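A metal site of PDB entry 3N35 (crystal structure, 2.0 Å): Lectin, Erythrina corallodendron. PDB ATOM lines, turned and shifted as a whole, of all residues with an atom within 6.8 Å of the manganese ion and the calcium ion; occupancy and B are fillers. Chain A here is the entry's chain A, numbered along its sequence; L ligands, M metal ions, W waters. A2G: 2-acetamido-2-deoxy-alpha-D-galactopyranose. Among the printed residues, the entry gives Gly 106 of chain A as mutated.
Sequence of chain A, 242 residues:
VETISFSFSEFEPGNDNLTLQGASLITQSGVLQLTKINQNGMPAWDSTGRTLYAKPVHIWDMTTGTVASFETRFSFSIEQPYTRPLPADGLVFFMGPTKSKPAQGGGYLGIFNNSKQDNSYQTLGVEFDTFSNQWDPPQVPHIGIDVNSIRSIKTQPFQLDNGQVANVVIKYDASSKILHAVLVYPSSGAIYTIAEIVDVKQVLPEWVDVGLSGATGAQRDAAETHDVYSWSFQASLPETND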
ATOM      1  N   ASP A  89      24.095  23.812  28.942  1.00  0.00           N
ATOM      2  CA  ASP A  89      22.707  24.214  28.722  1.00  0.00           C
ATOM      3  C   ASP A  89      22.064  24.783  29.996  1.00  0.00           C
ATOM      4  O   ASP A  89      21.096  25.545  29.930  1.00  0.00           O
ATOM      5  CB  ASP A  89      21.875  23.029  28.240  1.00  0.00           C
ATOM      6  CG  ASP A  89      21.827  22.936  26.731  1.00  0.00           C
ATOM      7  OD1 ASP A  89      21.181  23.803  26.104  1.00  0.00           O
ATOM      8  OD2 ASP A  89      22.442  22.005  26.173  1.00  0.00           O
ATOM      9  N   GLY A 106      20.785  18.058  26.888  1.00  0.00           N
ATOM     10  CA  GLY A 106      20.780  19.288  26.115  1.00  0.00           C
ATOM     11  C   GLY A 106      19.814  20.306  26.684  1.00  0.00           C
ATOM     12  O   GLY A 106      19.732  20.490  27.903  1.00  0.00           O
ATOM     13  N   GLY A 107      19.061  20.971  25.813  1.00  0.00           N
ATOM     14  CA  GLY A 107      18.107  21.978  26.236  1.00  0.00           C
ATOM     15  C   GLY A 107      16.960  21.478  27.101  1.00  0.00           C
ATOM     16  O   GLY A 107      16.212  22.286  27.654  1.00  0.00           O
ATOM     17  N   TYR A 108      16.795  20.163  27.196  1.00  0.00           N
ATOM     18  CA  TYR A 108      15.718  19.582  28.000  1.00  0.00           C
ATOM     19  C   TYR A 108      16.158  19.367  29.446  1.00  0.00           C
ATOM     20  O   TYR A 108      15.386  18.885  30.290  1.00  0.00           O
ATOM     21  CB  TYR A 108      15.254  18.269  27.372  1.00  0.00           C
ATOM     22  CG  TYR A 108      14.684  18.494  25.985  1.00  0.00           C
ATOM     23  CD1 TYR A 108      13.570  19.307  25.783  1.00  0.00           C
ATOM     24  CD2 TYR A 108      15.294  17.933  24.853  1.00  0.00           C
ATOM     25  CE1 TYR A 108      13.074  19.570  24.502  1.00  0.00           C
ATOM     26  CE2 TYR A 108      14.801  18.184  23.567  1.00  0.00           C
ATOM     27  CZ  TYR A 108      13.697  19.004  23.409  1.00  0.00           C
ATOM     28  OH  TYR A 108      13.227  19.275  22.144  1.00  0.00           O
ATOM     29  N   LEU A 109      17.409  19.721  29.708  1.00  0.00           N
ATOM     30  CA  LEU A 109      18.023  19.670  31.033  1.00  0.00           C
ATOM     31  C   LEU A 109      17.938  18.358  31.810  1.00  0.00           C
ATOM     32  O   LEU A 109      18.085  18.354  33.042  1.00  0.00           O
ATOM     33  CB  LEU A 109      17.449  20.808  31.892  1.00  0.00           C
ATOM     34  CG  LEU A 109      17.579  22.182  31.237  1.00  0.00           C
ATOM     35  CD1 LEU A 109      16.904  23.238  32.107  1.00  0.00           C
ATOM     36  CD2 LEU A 109      19.053  22.513  31.021  1.00  0.00           C
ATOM     37  N   GLU A 127      14.668  26.301  36.861  1.00  0.00           N
ATOM     38  CA  GLU A 127      15.875  26.245  36.047  1.00  0.00           C
ATOM     39  C   GLU A 127      16.737  27.496  36.052  1.00  0.00           C
ATOM     40  O   GLU A 127      16.270  28.611  36.300  1.00  0.00           O
ATOM     41  CB  GLU A 127      15.495  25.960  34.601  1.00  0.00           C
ATOM     42  CG  GLU A 127      14.602  27.053  34.009  1.00  0.00           C
ATOM     43  CD  GLU A 127      14.354  26.894  32.521  1.00  0.00           C
ATOM     44  OE1 GLU A 127      13.964  25.795  32.090  1.00  0.00           O
ATOM     45  OE2 GLU A 127      14.562  27.880  31.787  1.00  0.00           O
ATOM     46  N   ASP A 129      18.824  28.608  33.134  1.00  0.00           N
ATOM     47  CA  ASP A 129      19.063  28.357  31.730  1.00  0.00           C
ATOM     48  C   ASP A 129      20.128  29.230  31.071  1.00  0.00           C
ATOM     49  O   ASP A 129      19.981  30.447  31.054  1.00  0.00           O
ATOM     50  CB  ASP A 129      17.738  28.544  31.022  1.00  0.00           C
ATOM     51  CG  ASP A 129      17.674  27.838  29.717  1.00  0.00           C
ATOM     52  OD1 ASP A 129      18.740  27.656  29.085  1.00  0.00           O
ATOM     53  OD2 ASP A 129      16.552  27.472  29.309  1.00  0.00           O
ATOM     54  N   THR A 130      21.134  28.553  30.511  1.00  0.00           N
ATOM     55  CA  THR A 130      22.216  29.308  29.877  1.00  0.00           C
ATOM     56  C   THR A 130      22.244  29.387  28.350  1.00  0.00           C
ATOM     57  O   THR A 130      23.061  30.118  27.803  1.00  0.00           O
ATOM     58  CB  THR A 130      23.597  28.779  30.328  1.00  0.00           C
ATOM     59  OG1 THR A 130      23.674  27.380  30.060  1.00  0.00           O
ATOM     60  CG2 THR A 130      23.809  29.022  31.819  1.00  0.00           C
ATOM     61  N   PHE A 131      21.375  28.648  27.664  1.00  0.00           N
ATOM     62  CA  PHE A 131      21.360  28.662  26.203  1.00  0.00           C
ATOM     63  C   PHE A 131      19.961  28.944  25.703  1.00  0.00           C
ATOM     64  O   PHE A 131      19.014  28.341  26.167  1.00  0.00           O
ATOM     65  CB  PHE A 131      21.803  27.297  25.653  1.00  0.00           C
ATOM     66  CG  PHE A 131      21.858  27.251  24.156  1.00  0.00           C
ATOM     67  CD1 PHE A 131      22.996  27.656  23.465  1.00  0.00           C
ATOM     68  CD2 PHE A 131      20.750  26.802  23.419  1.00  0.00           C
ATOM     69  CE1 PHE A 131      23.035  27.635  22.065  1.00  0.00           C
ATOM     70  CE2 PHE A 131      20.787  26.784  22.028  1.00  0.00           C
ATOM     71  CZ  PHE A 131      21.930  27.203  21.345  1.00  0.00           C
ATOM     72  N   SER A 132      19.808  29.848  24.741  1.00  0.00           N
ATOM     73  CA  SER A 132      18.476  30.168  24.236  1.00  0.00           C
ATOM     74  C   SER A 132      17.963  29.229  23.140  1.00  0.00           C
ATOM     75  O   SER A 132      18.338  29.365  21.977  1.00  0.00           O
ATOM     76  CB  SER A 132      18.446  31.616  23.730  1.00  0.00           C
ATOM     77  OG  SER A 132      17.137  32.007  23.349  1.00  0.00           O
ATOM     78  N   ASN A 133      17.109  28.277  23.514  1.00  0.00           N
ATOM     79  CA  ASN A 133      16.526  27.356  22.535  1.00  0.00           C
ATOM     80  C   ASN A 133      15.354  28.049  21.843  1.00  0.00           C
ATOM     81  O   ASN A 133      14.990  29.168  22.184  1.00  0.00           O
ATOM     82  CB  ASN A 133      16.044  26.069  23.201  1.00  0.00           C
ATOM     83  CG  ASN A 133      17.178  25.234  23.758  1.00  0.00           C
ATOM     84  OD1 ASN A 133      17.582  25.414  24.897  1.00  0.00           O
ATOM     85  ND2 ASN A 133      17.709  24.327  22.947  1.00  0.00           N
ATOM     86  N   TRP A 135      12.297  27.627  22.147  1.00  0.00           N
ATOM     87  CA  TRP A 135      11.165  27.851  23.042  1.00  0.00           C
ATOM     88  C   TRP A 135      11.521  28.844  24.151  1.00  0.00           C
ATOM     89  O   TRP A 135      10.683  29.173  24.994  1.00  0.00           O
ATOM     90  CB  TRP A 135      10.737  26.537  23.679  1.00  0.00           C
ATOM     91  CG  TRP A 135      11.858  25.853  24.408  1.00  0.00           C
ATOM     92  CD1 TRP A 135      12.370  26.194  25.630  1.00  0.00           C
ATOM     93  CD2 TRP A 135      12.621  24.738  23.947  1.00  0.00           C
ATOM     94  NE1 TRP A 135      13.420  25.358  25.954  1.00  0.00           N
ATOM     95  CE2 TRP A 135      13.592  24.451  24.932  1.00  0.00           C
ATOM     96  CE3 TRP A 135      12.594  23.950  22.782  1.00  0.00           C
ATOM     97  CZ2 TRP A 135      14.518  23.414  24.798  1.00  0.00           C
ATOM     98  CZ3 TRP A 135      13.510  22.921  22.642  1.00  0.00           C
ATOM     99  CH2 TRP A 135      14.462  22.660  23.645  1.00  0.00           C
ATOM    100  N   ASP A 136      12.756  29.319  24.145  1.00  0.00           N
ATOM    101  CA  ASP A 136      13.228  30.242  25.158  1.00  0.00           C
ATOM    102  C   ASP A 136      13.138  31.706  24.816  1.00  0.00           C
ATOM    103  O   ASP A 136      12.992  32.080  23.650  1.00  0.00           O
ATOM    104  CB  ASP A 136      14.700  30.004  25.475  1.00  0.00           C
ATOM    105  CG  ASP A 136      14.927  28.812  26.342  1.00  0.00           C
ATOM    106  OD1 ASP A 136      14.083  28.525  27.206  1.00  0.00           O
ATOM    107  OD2 ASP A 136      15.976  28.179  26.164  1.00  0.00           O
ATOM    108  N   PRO A 137      13.224  32.563  25.841  1.00  0.00           N
ATOM    109  CA  PRO A 137      13.190  33.991  25.561  1.00  0.00           C
ATOM    110  C   PRO A 137      14.612  34.223  25.046  1.00  0.00           C
ATOM    111  O   PRO A 137      15.500  33.403  25.286  1.00  0.00           O
ATOM    112  CB  PRO A 137      12.951  34.610  26.942  1.00  0.00           C
ATOM    113  CG  PRO A 137      13.492  33.573  27.909  1.00  0.00           C
ATOM    114  CD  PRO A 137      13.035  32.281  27.275  1.00  0.00           C
ATOM    115  N   VAL A 140      19.662  35.210  27.944  1.00  0.00           N
ATOM    116  CA  VAL A 140      20.249  34.139  28.727  1.00  0.00           C
ATOM    117  C   VAL A 140      21.469  34.720  29.415  1.00  0.00           C
ATOM    118  O   VAL A 140      22.134  35.598  28.871  1.00  0.00           O
ATOM    119  CB  VAL A 140      20.670  32.915  27.878  1.00  0.00           C
ATOM    120  CG1 VAL A 140      19.455  32.086  27.522  1.00  0.00           C
ATOM    121  CG2 VAL A 140      21.401  33.373  26.623  1.00  0.00           C
ATOM    122  N   HIS A 142      18.743  32.856  32.224  1.00  0.00           N
ATOM    123  CA  HIS A 142      17.488  33.255  32.823  1.00  0.00           C
ATOM    124  C   HIS A 142      17.003  32.193  33.792  1.00  0.00           C
ATOM    125  O   HIS A 142      17.348  31.018  33.674  1.00  0.00           O
ATOM    126  CB  HIS A 142      16.401  33.515  31.771  1.00  0.00           C
ATOM    127  CG  HIS A 142      16.093  32.344  30.883  1.00  0.00           C
ATOM    128  ND1 HIS A 142      16.613  32.207  29.618  1.00  0.00           N
ATOM    129  CD2 HIS A 142      15.323  31.250  31.090  1.00  0.00           C
ATOM    130  CE1 HIS A 142      16.167  31.092  29.077  1.00  0.00           C
ATOM    131  NE2 HIS A 142      15.379  30.490  29.949  1.00  0.00           N
ATOM    132  N   ILE A 143      16.238  32.630  34.782  1.00  0.00           N
ATOM    133  CA  ILE A 143      15.652  31.721  35.755  1.00  0.00           C
ATOM    134  C   ILE A 143      14.286  31.447  35.146  1.00  0.00           C
ATOM    135  O   ILE A 143      13.680  32.333  34.557  1.00  0.00           O
ATOM    136  CB  ILE A 143      15.420  32.385  37.112  1.00  0.00           C
ATOM    137  CG1 ILE A 143      16.728  32.981  37.622  1.00  0.00           C
ATOM    138  CG2 ILE A 143      14.872  31.349  38.109  1.00  0.00           C
ATOM    139  CD1 ILE A 143      16.584  33.958  38.792  1.00  0.00           C
ATOM    140  N   GLY A 144      13.792  30.226  35.290  1.00  0.00           N
ATOM    141  CA  GLY A 144      12.490  29.928  34.740  1.00  0.00           C
ATOM    142  C   GLY A 144      11.720  28.980  35.632  1.00  0.00           C
ATOM    143  O   GLY A 144      12.319  28.170  36.335  1.00  0.00           O
ATOM    144  N   ASP A 146       9.252  26.001  35.438  1.00  0.00           N
ATOM    145  CA  ASP A 146       8.745  25.039  34.473  1.00  0.00           C
ATOM    146  C   ASP A 146       7.687  24.135  35.080  1.00  0.00           C
ATOM    147  O   ASP A 146       7.934  23.431  36.063  1.00  0.00           O
ATOM    148  CB  ASP A 146       9.886  24.167  33.934  1.00  0.00           C
ATOM    149  CG  ASP A 146      11.020  24.994  33.333  1.00  0.00           C
ATOM    150  OD1 ASP A 146      10.801  26.188  33.051  1.00  0.00           O
ATOM    151  OD2 ASP A 146      12.124  24.434  33.133  1.00  0.00           O
ATOM    152  N   ILE A 150       9.231  22.401  29.234  1.00  0.00           N
ATOM    153  CA  ILE A 150      10.523  23.075  29.227  1.00  0.00           C
ATOM    154  C   ILE A 150      10.274  24.547  28.892  1.00  0.00           C
ATOM    155  O   ILE A 150      11.128  25.416  29.109  1.00  0.00           O
ATOM    156  CB  ILE A 150      11.482  22.425  28.194  1.00  0.00           C
ATOM    157  CG1 ILE A 150      12.913  22.930  28.409  1.00  0.00           C
ATOM    158  CG2 ILE A 150      10.993  22.692  26.782  1.00  0.00           C
ATOM    159  CD1 ILE A 150      13.618  22.379  29.643  1.00  0.00           C
ATOM    160  N   ARG A 151       9.097  24.829  28.335  1.00  0.00           N
ATOM    161  CA  ARG A 151       8.705  26.185  27.989  1.00  0.00           C
ATOM    162  C   ARG A 151       8.135  26.781  29.285  1.00  0.00           C
ATOM    163  O   ARG A 151       7.003  26.477  29.677  1.00  0.00           O
ATOM    164  CB  ARG A 151       7.654  26.156  26.876  1.00  0.00           C
ATOM    165  CG  ARG A 151       7.202  27.534  26.406  1.00  0.00           C
ATOM    166  CD  ARG A 151       6.180  27.450  25.254  1.00  0.00           C
ATOM    167  NE  ARG A 151       6.792  27.442  23.936  1.00  0.00           N
ATOM    168  CZ  ARG A 151       7.056  26.349  23.215  1.00  0.00           C
ATOM    169  NH1 ARG A 151       6.766  25.149  23.696  1.00  0.00           N
ATOM    170  NH2 ARG A 151       7.601  26.464  22.009  1.00  0.00           N
ATOM    171  N   SER A 152       8.929  27.613  29.950  1.00  0.00           N
ATOM    172  CA  SER A 152       8.548  28.221  31.229  1.00  0.00           C
ATOM    173  C   SER A 152       7.275  29.049  31.218  1.00  0.00           C
ATOM    174  O   SER A 152       6.948  29.697  30.221  1.00  0.00           O
ATOM    175  CB  SER A 152       9.701  29.093  31.739  1.00  0.00           C
ATOM    176  OG  SER A 152      10.937  28.397  31.713  1.00  0.00           O
ATOM    177  N   THR A 155       9.768  33.684  33.288  1.00  0.00           N
ATOM    178  CA  THR A 155      11.221  33.753  33.292  1.00  0.00           C
ATOM    179  C   THR A 155      11.724  35.092  33.812  1.00  0.00           C
ATOM    180  O   THR A 155      11.003  36.092  33.798  1.00  0.00           O
ATOM    181  CB  THR A 155      11.807  33.536  31.886  1.00  0.00           C
ATOM    182  OG1 THR A 155      11.319  34.541  30.991  1.00  0.00           O
ATOM    183  CG2 THR A 155      11.426  32.163  31.358  1.00  0.00           C
HETATM  184  O5  A2G L   1      22.871  22.118  20.931  1.00  0.00           O
HETATM  185  C1  A2G L   1      21.516  21.824  20.574  1.00  0.00           C
HETATM  186  O1  A2G L   1      21.049  22.869  19.692  1.00  0.00           O
HETATM  187  C2  A2G L   1      20.688  21.791  21.868  1.00  0.00           C
HETATM  188  N2  A2G L   1      19.287  21.674  21.478  1.00  0.00           N
HETATM  189  C3  A2G L   1      20.821  23.127  22.614  1.00  0.00           C
HETATM  190  O3  A2G L   1      20.186  23.029  23.887  1.00  0.00           O
HETATM  191  C4  A2G L   1      22.291  23.490  22.814  1.00  0.00           C
HETATM  192  O4  A2G L   1      22.876  22.533  23.698  1.00  0.00           O
HETATM  193  C5  A2G L   1      23.030  23.425  21.485  1.00  0.00           C
HETATM  194  C6  A2G L   1      24.522  23.703  21.656  1.00  0.00           C
HETATM  195  O6  A2G L   1      24.897  24.538  20.572  1.00  0.00           O
HETATM  196  C7  A2G L   1      18.459  20.807  22.093  1.00  0.00           C
HETATM  197  O7  A2G L   1      18.819  20.077  23.007  1.00  0.00           O
HETATM  198  C8  A2G L   1      17.043  20.778  21.601  1.00  0.00           C
HETATM  199 MN    MN M   1      14.441  28.395  29.532  1.00  0.00          MN
HETATM  200 CA    CA M   2      17.524  26.601  27.116  1.00  0.00          CA
HETATM  201  O   HOH W   1      15.828  24.810  27.958  1.00  0.00           O
HETATM  202  O   HOH W   2      19.532  25.027  27.768  1.00  0.00           O
HETATM  203  O   HOH W   3      13.679  26.155  29.284  1.00  0.00           O
HETATM  204  O   HOH W   4      12.199  29.244  29.656  1.00  0.00           O
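The side-chain amide nitrogen of Asn 133 sits at hydrogen-bond distance from an oxygen (O3) of the ligand (3.0 Å). O7 of the ligand sits at hydrogen-bond distance from N of Gly 107, 3.0 Å away. An oxygen (O3) of the ligand lies within hydrogen-bond range of the side-chain carboxylate (OD1) of Asp 89 (2.6 Å).
OE1 of Glu 127 sits close to OD2 of Asp 146 (2.5 Å). The backbone NH of Glu 127 sits at hydrogen-bond distance from the backbone carbonyl oxygen of Gly 144 (3.0 Å). The side-chain carboxylate (OD1) of Asp 136 lies close to the indole nitrogen (NE1) of Trp 135.
Of the 23 residues printed, 4 come within 4 Å of the calcium ion. The nearest printed residue that does not touch the calcium ion is Trp 135 (4.4 Å).
The manganese ion is bound by the side-chain carboxylate of Asp 129, the side-chain carboxylate of Glu 127, a ring nitrogen (NE2) of His 142, the side-chain carboxylate of Asp 136, water W3 and water W4. The manganese ion has six donor atoms within binding distance.
The side-chain carboxylate (OD2) of Asp 136 is bound to the calcium ion, at 2.4 Å. The calcium ion is bound by O of Phe 131. OD1 of Asn 133 is bound to the calcium ion, at 2.5 Å. The calcium ion is bound by the side-chain carboxylate (OD1) of Asp 129. OD2 of Asp 129 binds the calcium ion (2.6 Å). The calcium ion is bound by water W1 (2.6 Å). Water W2 binds the calcium ion. The calcium ion has seven donor atoms within binding distance.
Water W3 lies within hydrogen-bond range of O of Ile 150, OE1 of Glu 127 and NE1 of Trp 135. Water W1 bridges O of Gly 107 (2.6 Å) and NE1 of Trp 135 (3.2 Å).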
